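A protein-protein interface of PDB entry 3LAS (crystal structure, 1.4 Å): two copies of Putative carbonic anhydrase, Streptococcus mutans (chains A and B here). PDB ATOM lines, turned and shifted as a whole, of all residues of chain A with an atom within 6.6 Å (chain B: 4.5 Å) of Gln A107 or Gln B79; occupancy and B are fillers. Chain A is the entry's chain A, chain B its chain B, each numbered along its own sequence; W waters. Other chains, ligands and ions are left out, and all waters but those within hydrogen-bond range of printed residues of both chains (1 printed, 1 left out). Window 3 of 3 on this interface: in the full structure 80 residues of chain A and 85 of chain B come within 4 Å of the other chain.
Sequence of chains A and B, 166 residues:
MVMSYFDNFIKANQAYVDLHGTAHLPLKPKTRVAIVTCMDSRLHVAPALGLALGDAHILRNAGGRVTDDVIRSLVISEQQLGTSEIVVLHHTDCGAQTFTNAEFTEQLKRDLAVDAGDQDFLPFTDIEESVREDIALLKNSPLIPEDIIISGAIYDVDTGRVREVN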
ATOM      1  N   ALA A 102      -9.535  12.150  13.833  1.00  0.00           N
ATOM      2  CA  ALA A 102     -10.508  11.292  13.201  1.00  0.00           C
ATOM      3  C   ALA A 102     -11.510  10.689  14.171  1.00  0.00           C
ATOM      4  O   ALA A 102     -12.684  10.716  13.920  1.00  0.00           O
ATOM      5  CB  ALA A 102      -9.719  10.161  12.428  1.00  0.00           C
ATOM      6  N   GLU A 103     -11.039  10.233  15.300  1.00  0.00           N
ATOM      7  CA  GLU A 103     -11.939   9.565  16.282  1.00  0.00           C
ATOM      8  C   GLU A 103     -12.848  10.669  16.880  1.00  0.00           C
ATOM      9  O   GLU A 103     -14.054  10.478  17.041  1.00  0.00           O
ATOM     10  CB  GLU A 103     -11.118   9.058  17.506  1.00  0.00           C
ATOM     11  CG  GLU A 103     -10.032   8.005  17.290  1.00  0.00           C
ATOM     12  CD  GLU A 103      -9.186   7.717  18.562  1.00  0.00           C
ATOM     13  OE1 GLU A 103      -8.935   8.669  19.456  1.00  0.00           O
ATOM     14  OE2 GLU A 103      -8.785   6.529  18.624  1.00  0.00           O
ATOM     15  N   PHE A 104     -12.283  11.848  17.169  1.00  0.00           N
ATOM     16  CA  PHE A 104     -13.064  12.873  17.881  1.00  0.00           C
ATOM     17  C   PHE A 104     -14.121  13.432  16.949  1.00  0.00           C
ATOM     18  O   PHE A 104     -15.250  13.630  17.308  1.00  0.00           O
ATOM     19  CB  PHE A 104     -12.143  13.933  18.387  1.00  0.00           C
ATOM     20  CG  PHE A 104     -12.809  14.875  19.322  1.00  0.00           C
ATOM     21  CD1 PHE A 104     -12.649  16.216  19.167  1.00  0.00           C
ATOM     22  CD2 PHE A 104     -13.514  14.465  20.466  1.00  0.00           C
ATOM     23  CE1 PHE A 104     -13.181  17.137  20.069  1.00  0.00           C
ATOM     24  CE2 PHE A 104     -14.049  15.438  21.378  1.00  0.00           C
ATOM     25  CZ  PHE A 104     -13.916  16.765  21.125  1.00  0.00           C
ATOM     26  N   THR A 105     -13.795  13.589  15.661  1.00  0.00           N
ATOM     27  CA  THR A 105     -14.743  14.225  14.759  1.00  0.00           C
ATOM     28  C   THR A 105     -15.836  13.181  14.477  1.00  0.00           C
ATOM     29  O   THR A 105     -17.016  13.554  14.357  1.00  0.00           O
ATOM     30  CB  THR A 105     -14.019  14.939  13.472  1.00  0.00           C
ATOM     31  OG1 THR A 105     -13.411  13.871  12.863  1.00  0.00           O
ATOM     32  CG2 THR A 105     -13.064  15.998  13.926  1.00  0.00           C
ATOM     33  N   GLU A 106     -15.529  11.882  14.506  1.00  0.00           N
ATOM     34  CA  GLU A 106     -16.649  10.911  14.399  1.00  0.00           C
ATOM     35  C   GLU A 106     -17.591  11.010  15.618  1.00  0.00           C
ATOM     36  O   GLU A 106     -18.840  10.912  15.473  1.00  0.00           O
ATOM     37  CB  GLU A 106     -16.126   9.485  14.293  1.00  0.00           C
ATOM     38  CG  GLU A 106     -15.566   9.146  12.908  1.00  0.00           C
ATOM     39  CD  GLU A 106     -16.535   9.552  11.808  1.00  0.00           C
ATOM     40  OE1 GLU A 106     -17.665   8.980  11.759  1.00  0.00           O
ATOM     41  OE2 GLU A 106     -16.160  10.463  11.004  1.00  0.00           O
ATOM     42  N   GLN A 107     -17.006  11.141  16.854  1.00  0.00           N
ATOM     43  CA  GLN A 107     -17.786  11.304  18.008  1.00  0.00           C
ATOM     44  C   GLN A 107     -18.675  12.543  17.959  1.00  0.00           C
ATOM     45  O   GLN A 107     -19.872  12.511  18.339  1.00  0.00           O
ATOM     46  CB  GLN A 107     -16.856  11.399  19.215  1.00  0.00           C
ATOM     47  CG  GLN A 107     -17.603  11.508  20.600  1.00  0.00           C
ATOM     48  CD  GLN A 107     -16.666  11.697  21.745  1.00  0.00           C
ATOM     49  OE1 GLN A 107     -16.832  12.615  22.632  1.00  0.00           O
ATOM     50  NE2 GLN A 107     -15.636  10.905  21.763  1.00  0.00           N
ATOM     51  N   LEU A 108     -18.149  13.676  17.468  1.00  0.00           N
ATOM     52  CA  LEU A 108     -18.956  14.855  17.342  1.00  0.00           C
ATOM     53  C   LEU A 108     -20.105  14.675  16.347  1.00  0.00           C
ATOM     54  O   LEU A 108     -21.190  15.220  16.556  1.00  0.00           O
ATOM     55  CB  LEU A 108     -18.109  16.060  16.985  1.00  0.00           C
ATOM     56  CG  LEU A 108     -17.011  16.364  17.996  1.00  0.00           C
ATOM     57  CD1 LEU A 108     -16.221  17.536  17.479  1.00  0.00           C
ATOM     58  CD2 LEU A 108     -17.517  16.777  19.408  1.00  0.00           C
ATOM     59  N   LYS A 109     -19.860  13.974  15.260  1.00  0.00           N
ATOM     60  CA  LYS A 109     -20.931  13.746  14.276  1.00  0.00           C
ATOM     61  C   LYS A 109     -22.042  12.955  14.967  1.00  0.00           C
ATOM     62  O   LYS A 109     -23.225  13.293  14.819  1.00  0.00           O
ATOM     63  CB  LYS A 109     -20.378  12.933  13.102  1.00  0.00           C
ATOM     64  CG  LYS A 109     -19.678  13.628  12.038  1.00  0.00           C
ATOM     65  N   ARG A 110     -21.694  11.939  15.715  1.00  0.00           N
ATOM     66  CA  ARG A 110     -22.720  11.076  16.417  1.00  0.00           C
ATOM     67  C   ARG A 110     -23.453  11.872  17.460  1.00  0.00           C
ATOM     68  O   ARG A 110     -24.681  11.789  17.562  1.00  0.00           O
ATOM     69  CB  ARG A 110     -22.060   9.888  17.097  1.00  0.00           C
ATOM     70  CG  ARG A 110     -21.509   8.836  16.131  1.00  0.00           C
ATOM     71  CD  ARG A 110     -21.048   7.563  16.909  1.00  0.00           C
ATOM     72  NE  ARG A 110     -19.975   7.794  17.922  1.00  0.00           N
ATOM     73  CZ  ARG A 110     -18.656   7.672  17.661  1.00  0.00           C
ATOM     74  NH1 ARG A 110     -18.268   7.281  16.447  1.00  0.00           N
ATOM     75  NH2 ARG A 110     -17.761   7.862  18.613  1.00  0.00           N
ATOM     76  N   ASP A 111     -22.742  12.656  18.239  1.00  0.00           N
ATOM     77  CA  ASP A 111     -23.337  13.284  19.411  1.00  0.00           C
ATOM     78  C   ASP A 111     -23.962  14.649  19.175  1.00  0.00           C
ATOM     79  O   ASP A 111     -24.959  15.011  19.845  1.00  0.00           O
ATOM     80  CB  ASP A 111     -22.326  13.432  20.536  1.00  0.00           C
ATOM     81  CG  ASP A 111     -21.880  12.090  21.092  1.00  0.00           C
ATOM     82  OD1 ASP A 111     -22.502  11.040  20.765  1.00  0.00           O
ATOM     83  OD2 ASP A 111     -20.971  11.958  21.931  1.00  0.00           O
ATOM     84  N   LEU A 112     -23.370  15.447  18.306  1.00  0.00           N
ATOM     85  CA  LEU A 112     -23.813  16.813  18.058  1.00  0.00           C
ATOM     86  C   LEU A 112     -24.411  16.989  16.665  1.00  0.00           C
ATOM     87  O   LEU A 112     -24.861  18.116  16.368  1.00  0.00           O
ATOM     88  CB  LEU A 112     -22.671  17.817  18.227  1.00  0.00           C
ATOM     89  CG  LEU A 112     -21.956  17.817  19.580  1.00  0.00           C
ATOM     90  CD1 LEU A 112     -21.049  19.015  19.601  1.00  0.00           C
ATOM     91  CD2 LEU A 112     -22.869  17.669  20.789  1.00  0.00           C
ATOM     92  N   ALA A 113     -24.295  15.972  15.819  1.00  0.00           N
ATOM     93  CA  ALA A 113     -24.800  16.137  14.417  1.00  0.00           C
ATOM     94  C   ALA A 113     -24.136  17.278  13.680  1.00  0.00           C
ATOM     95  O   ALA A 113     -24.756  18.019  12.896  1.00  0.00           O
ATOM     96  CB  ALA A 113     -26.372  16.276  14.370  1.00  0.00           C
ATOM     97  N   VAL A 114     -22.852  17.477  13.952  1.00  0.00           N
ATOM     98  CA  VAL A 114     -22.068  18.459  13.239  1.00  0.00           C
ATOM     99  C   VAL A 114     -20.936  17.685  12.620  1.00  0.00           C
ATOM    100  O   VAL A 114     -20.327  16.802  13.275  1.00  0.00           O
ATOM    101  CB  VAL A 114     -21.429  19.494  14.163  1.00  0.00           C
ATOM    102  CG1 VAL A 114     -22.514  20.452  14.748  1.00  0.00           C
ATOM    103  CG2 VAL A 114     -20.591  18.730  15.150  1.00  0.00           C
ATOM    104  N   VAL B  75     -15.021  22.698  23.000  1.00  0.00           N
ATOM    105  CA  VAL B  75     -15.568  21.429  22.535  1.00  0.00           C
ATOM    106  C   VAL B  75     -14.713  20.292  23.153  1.00  0.00           C
ATOM    107  O   VAL B  75     -15.251  19.259  23.562  1.00  0.00           O
ATOM    108  CB  VAL B  75     -15.473  21.400  20.993  1.00  0.00           C
ATOM    109  CG1 VAL B  75     -15.751  19.943  20.462  1.00  0.00           C
ATOM    110  CG2 VAL B  75     -16.471  22.408  20.465  1.00  0.00           C
ATOM    111  N   ILE B  76     -13.405  20.450  23.213  1.00  0.00           N
ATOM    112  CA  ILE B  76     -12.565  19.446  23.904  1.00  0.00           C
ATOM    113  C   ILE B  76     -12.957  19.388  25.363  1.00  0.00           C
ATOM    114  O   ILE B  76     -13.174  18.281  25.932  1.00  0.00           O
ATOM    115  CB  ILE B  76     -11.056  19.734  23.702  1.00  0.00           C
ATOM    116  CG1 ILE B  76     -10.713  19.532  22.219  1.00  0.00           C
ATOM    117  CG2 ILE B  76     -10.207  18.877  24.639  1.00  0.00           C
ATOM    118  CD1 ILE B  76      -9.377  20.194  21.873  1.00  0.00           C
ATOM    119  N   SER B  77     -13.046  20.518  26.055  1.00  0.00           N
ATOM    120  CA  SER B  77     -13.397  20.515  27.488  1.00  0.00           C
ATOM    121  C   SER B  77     -14.719  19.816  27.723  1.00  0.00           C
ATOM    122  O   SER B  77     -14.827  19.076  28.738  1.00  0.00           O
ATOM    123  CB  SER B  77     -13.540  21.978  27.888  1.00  0.00           C
ATOM    124  OG  SER B  77     -13.902  22.113  29.247  1.00  0.00           O
ATOM    125  N   GLU B  78     -15.723  20.036  26.884  1.00  0.00           N
ATOM    126  CA  GLU B  78     -17.068  19.512  27.099  1.00  0.00           C
ATOM    127  C   GLU B  78     -17.198  18.104  26.564  1.00  0.00           C
ATOM    128  O   GLU B  78     -17.681  17.217  27.304  1.00  0.00           O
ATOM    129  CB  GLU B  78     -18.057  20.430  26.388  1.00  0.00           C
ATOM    130  CG  GLU B  78     -18.113  21.825  27.121  1.00  0.00           C
ATOM    131  CD  GLU B  78     -18.933  22.840  26.440  1.00  0.00           C
ATOM    132  OE1 GLU B  78     -19.467  22.698  25.316  1.00  0.00           O
ATOM    133  OE2 GLU B  78     -19.022  23.965  27.045  1.00  0.00           O
ATOM    134  N   GLN B  79     -16.867  17.832  25.316  1.00  0.00           N
ATOM    135  CA  GLN B  79     -17.162  16.566  24.695  1.00  0.00           C
ATOM    136  C   GLN B  79     -16.102  15.553  25.018  1.00  0.00           C
ATOM    137  O   GLN B  79     -16.433  14.324  25.053  1.00  0.00           O
ATOM    138  CB  GLN B  79     -17.228  16.740  23.149  1.00  0.00           C
ATOM    139  CG  GLN B  79     -18.330  17.747  22.760  1.00  0.00           C
ATOM    140  CD  GLN B  79     -19.657  17.484  23.459  1.00  0.00           C
ATOM    141  OE1 GLN B  79     -20.119  16.344  23.514  1.00  0.00           O
ATOM    142  NE2 GLN B  79     -20.272  18.561  23.917  1.00  0.00           N
ATOM    143  N   GLN B  80     -14.848  15.906  25.260  1.00  0.00           N
ATOM    144  CA  GLN B  80     -13.851  14.940  25.676  1.00  0.00           C
ATOM    145  C   GLN B  80     -13.650  14.900  27.126  1.00  0.00           C
ATOM    146  O   GLN B  80     -13.324  13.800  27.667  1.00  0.00           O
ATOM    147  CB  GLN B  80     -12.515  15.214  24.942  1.00  0.00           C
ATOM    148  CG  GLN B  80     -11.364  14.211  25.135  1.00  0.00           C
ATOM    149  CD  GLN B  80     -11.654  12.876  24.461  1.00  0.00           C
ATOM    150  OE1 GLN B  80     -12.694  12.650  23.846  1.00  0.00           O
ATOM    151  NE2 GLN B  80     -10.705  11.982  24.626  1.00  0.00           N
ATOM    152  N   LEU B  81     -13.746  16.005  27.850  1.00  0.00           N
ATOM    153  CA  LEU B  81     -13.302  16.049  29.276  1.00  0.00           C
ATOM    154  C   LEU B  81     -14.387  16.352  30.189  1.00  0.00           C
ATOM    155  O   LEU B  81     -14.119  16.652  31.353  1.00  0.00           O
ATOM    156  CB  LEU B  81     -12.088  17.046  29.389  1.00  0.00           C
ATOM    157  CG  LEU B  81     -10.880  16.750  28.469  1.00  0.00           C
ATOM    158  CD1 LEU B  81      -9.818  17.880  28.658  1.00  0.00           C
ATOM    159  CD2 LEU B  81     -10.214  15.403  28.779  1.00  0.00           C
ATOM    160  N   PRO B 145     -23.521  22.588  22.831  1.00  0.00           N
ATOM    161  CA  PRO B 145     -24.930  22.093  22.899  1.00  0.00           C
ATOM    162  C   PRO B 145     -25.765  23.134  23.631  1.00  0.00           C
ATOM    163  O   PRO B 145     -25.339  23.898  24.557  1.00  0.00           O
ATOM    164  CB  PRO B 145     -24.819  20.810  23.759  1.00  0.00           C
ATOM    165  CG  PRO B 145     -23.378  20.299  23.423  1.00  0.00           C
ATOM    166  CD  PRO B 145     -22.549  21.539  23.250  1.00  0.00           C
HETATM  167  O   HOH W   1     -12.752  11.336  21.343  1.00  0.00           O
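The side-chain amide oxygen (OE1) of Gln A107 sits close to the backbone carbonyl oxygen (O) of Gln B79 (3.0 Å).
N of Ala A113 is in hydrogen-bond range of O of Leu A108 (3.3 Å).
Among the printed residues, pairs that only touch across the chains: Leu A108 with Gln B79, Phe A104 with Val B75, Leu A112 with Pro B145, Leu A108 with Val B75, Phe A104 with Gln B79 and Phe A104 with Gln B80.
Of the printed residues of chain B, Gln A107 touches Gln B79.
Of the printed residues of chain A, Gln B79 touches Phe A104, Gln A107 and Leu A108.
Of the printed residues of chain A, Pro B145 touches Leu A112 (3.8 Å).
Printed residues of chain A within 4 Å of Gln B80: Phe A104 (3.9 Å).
Of the printed residues of chain B, Phe A104 touches Val B75, Gln B79 and Gln B80.
The nearest printed residue of chain B that does not touch Gln A107 is Gln B80 (4.005 Å).
The nearest printed residue of chain A that does not touch Pro B145 is Asp A111 (6.6 Å).
Of the 13 printed residues of chain A, 4 touch a printed residue of chain B.
Hydrophobic or aromatic side chains of chain A within 4 Å of the printed part of chain B: Phe A104, Leu A108 and Leu A112.
Printed residues of chain B that touch a printed residue of chain A: Val B75, Gln B79, Gln B80 and Pro B145.
Hydrophobic or aromatic side chains of chain B within 4 Å of the printed part of chain A: Val B75 and Pro B145.
Among the printed residues, no Asp or Glu carboxylate lies within 4 Å of a Lys or Arg side-chain nitrogen of the other chain.
No position is printed for both chains.
Water W1 bridges OE1 of Gln B80 (2.8 Å) and NE2 of Gln A107 (2.9 Å).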
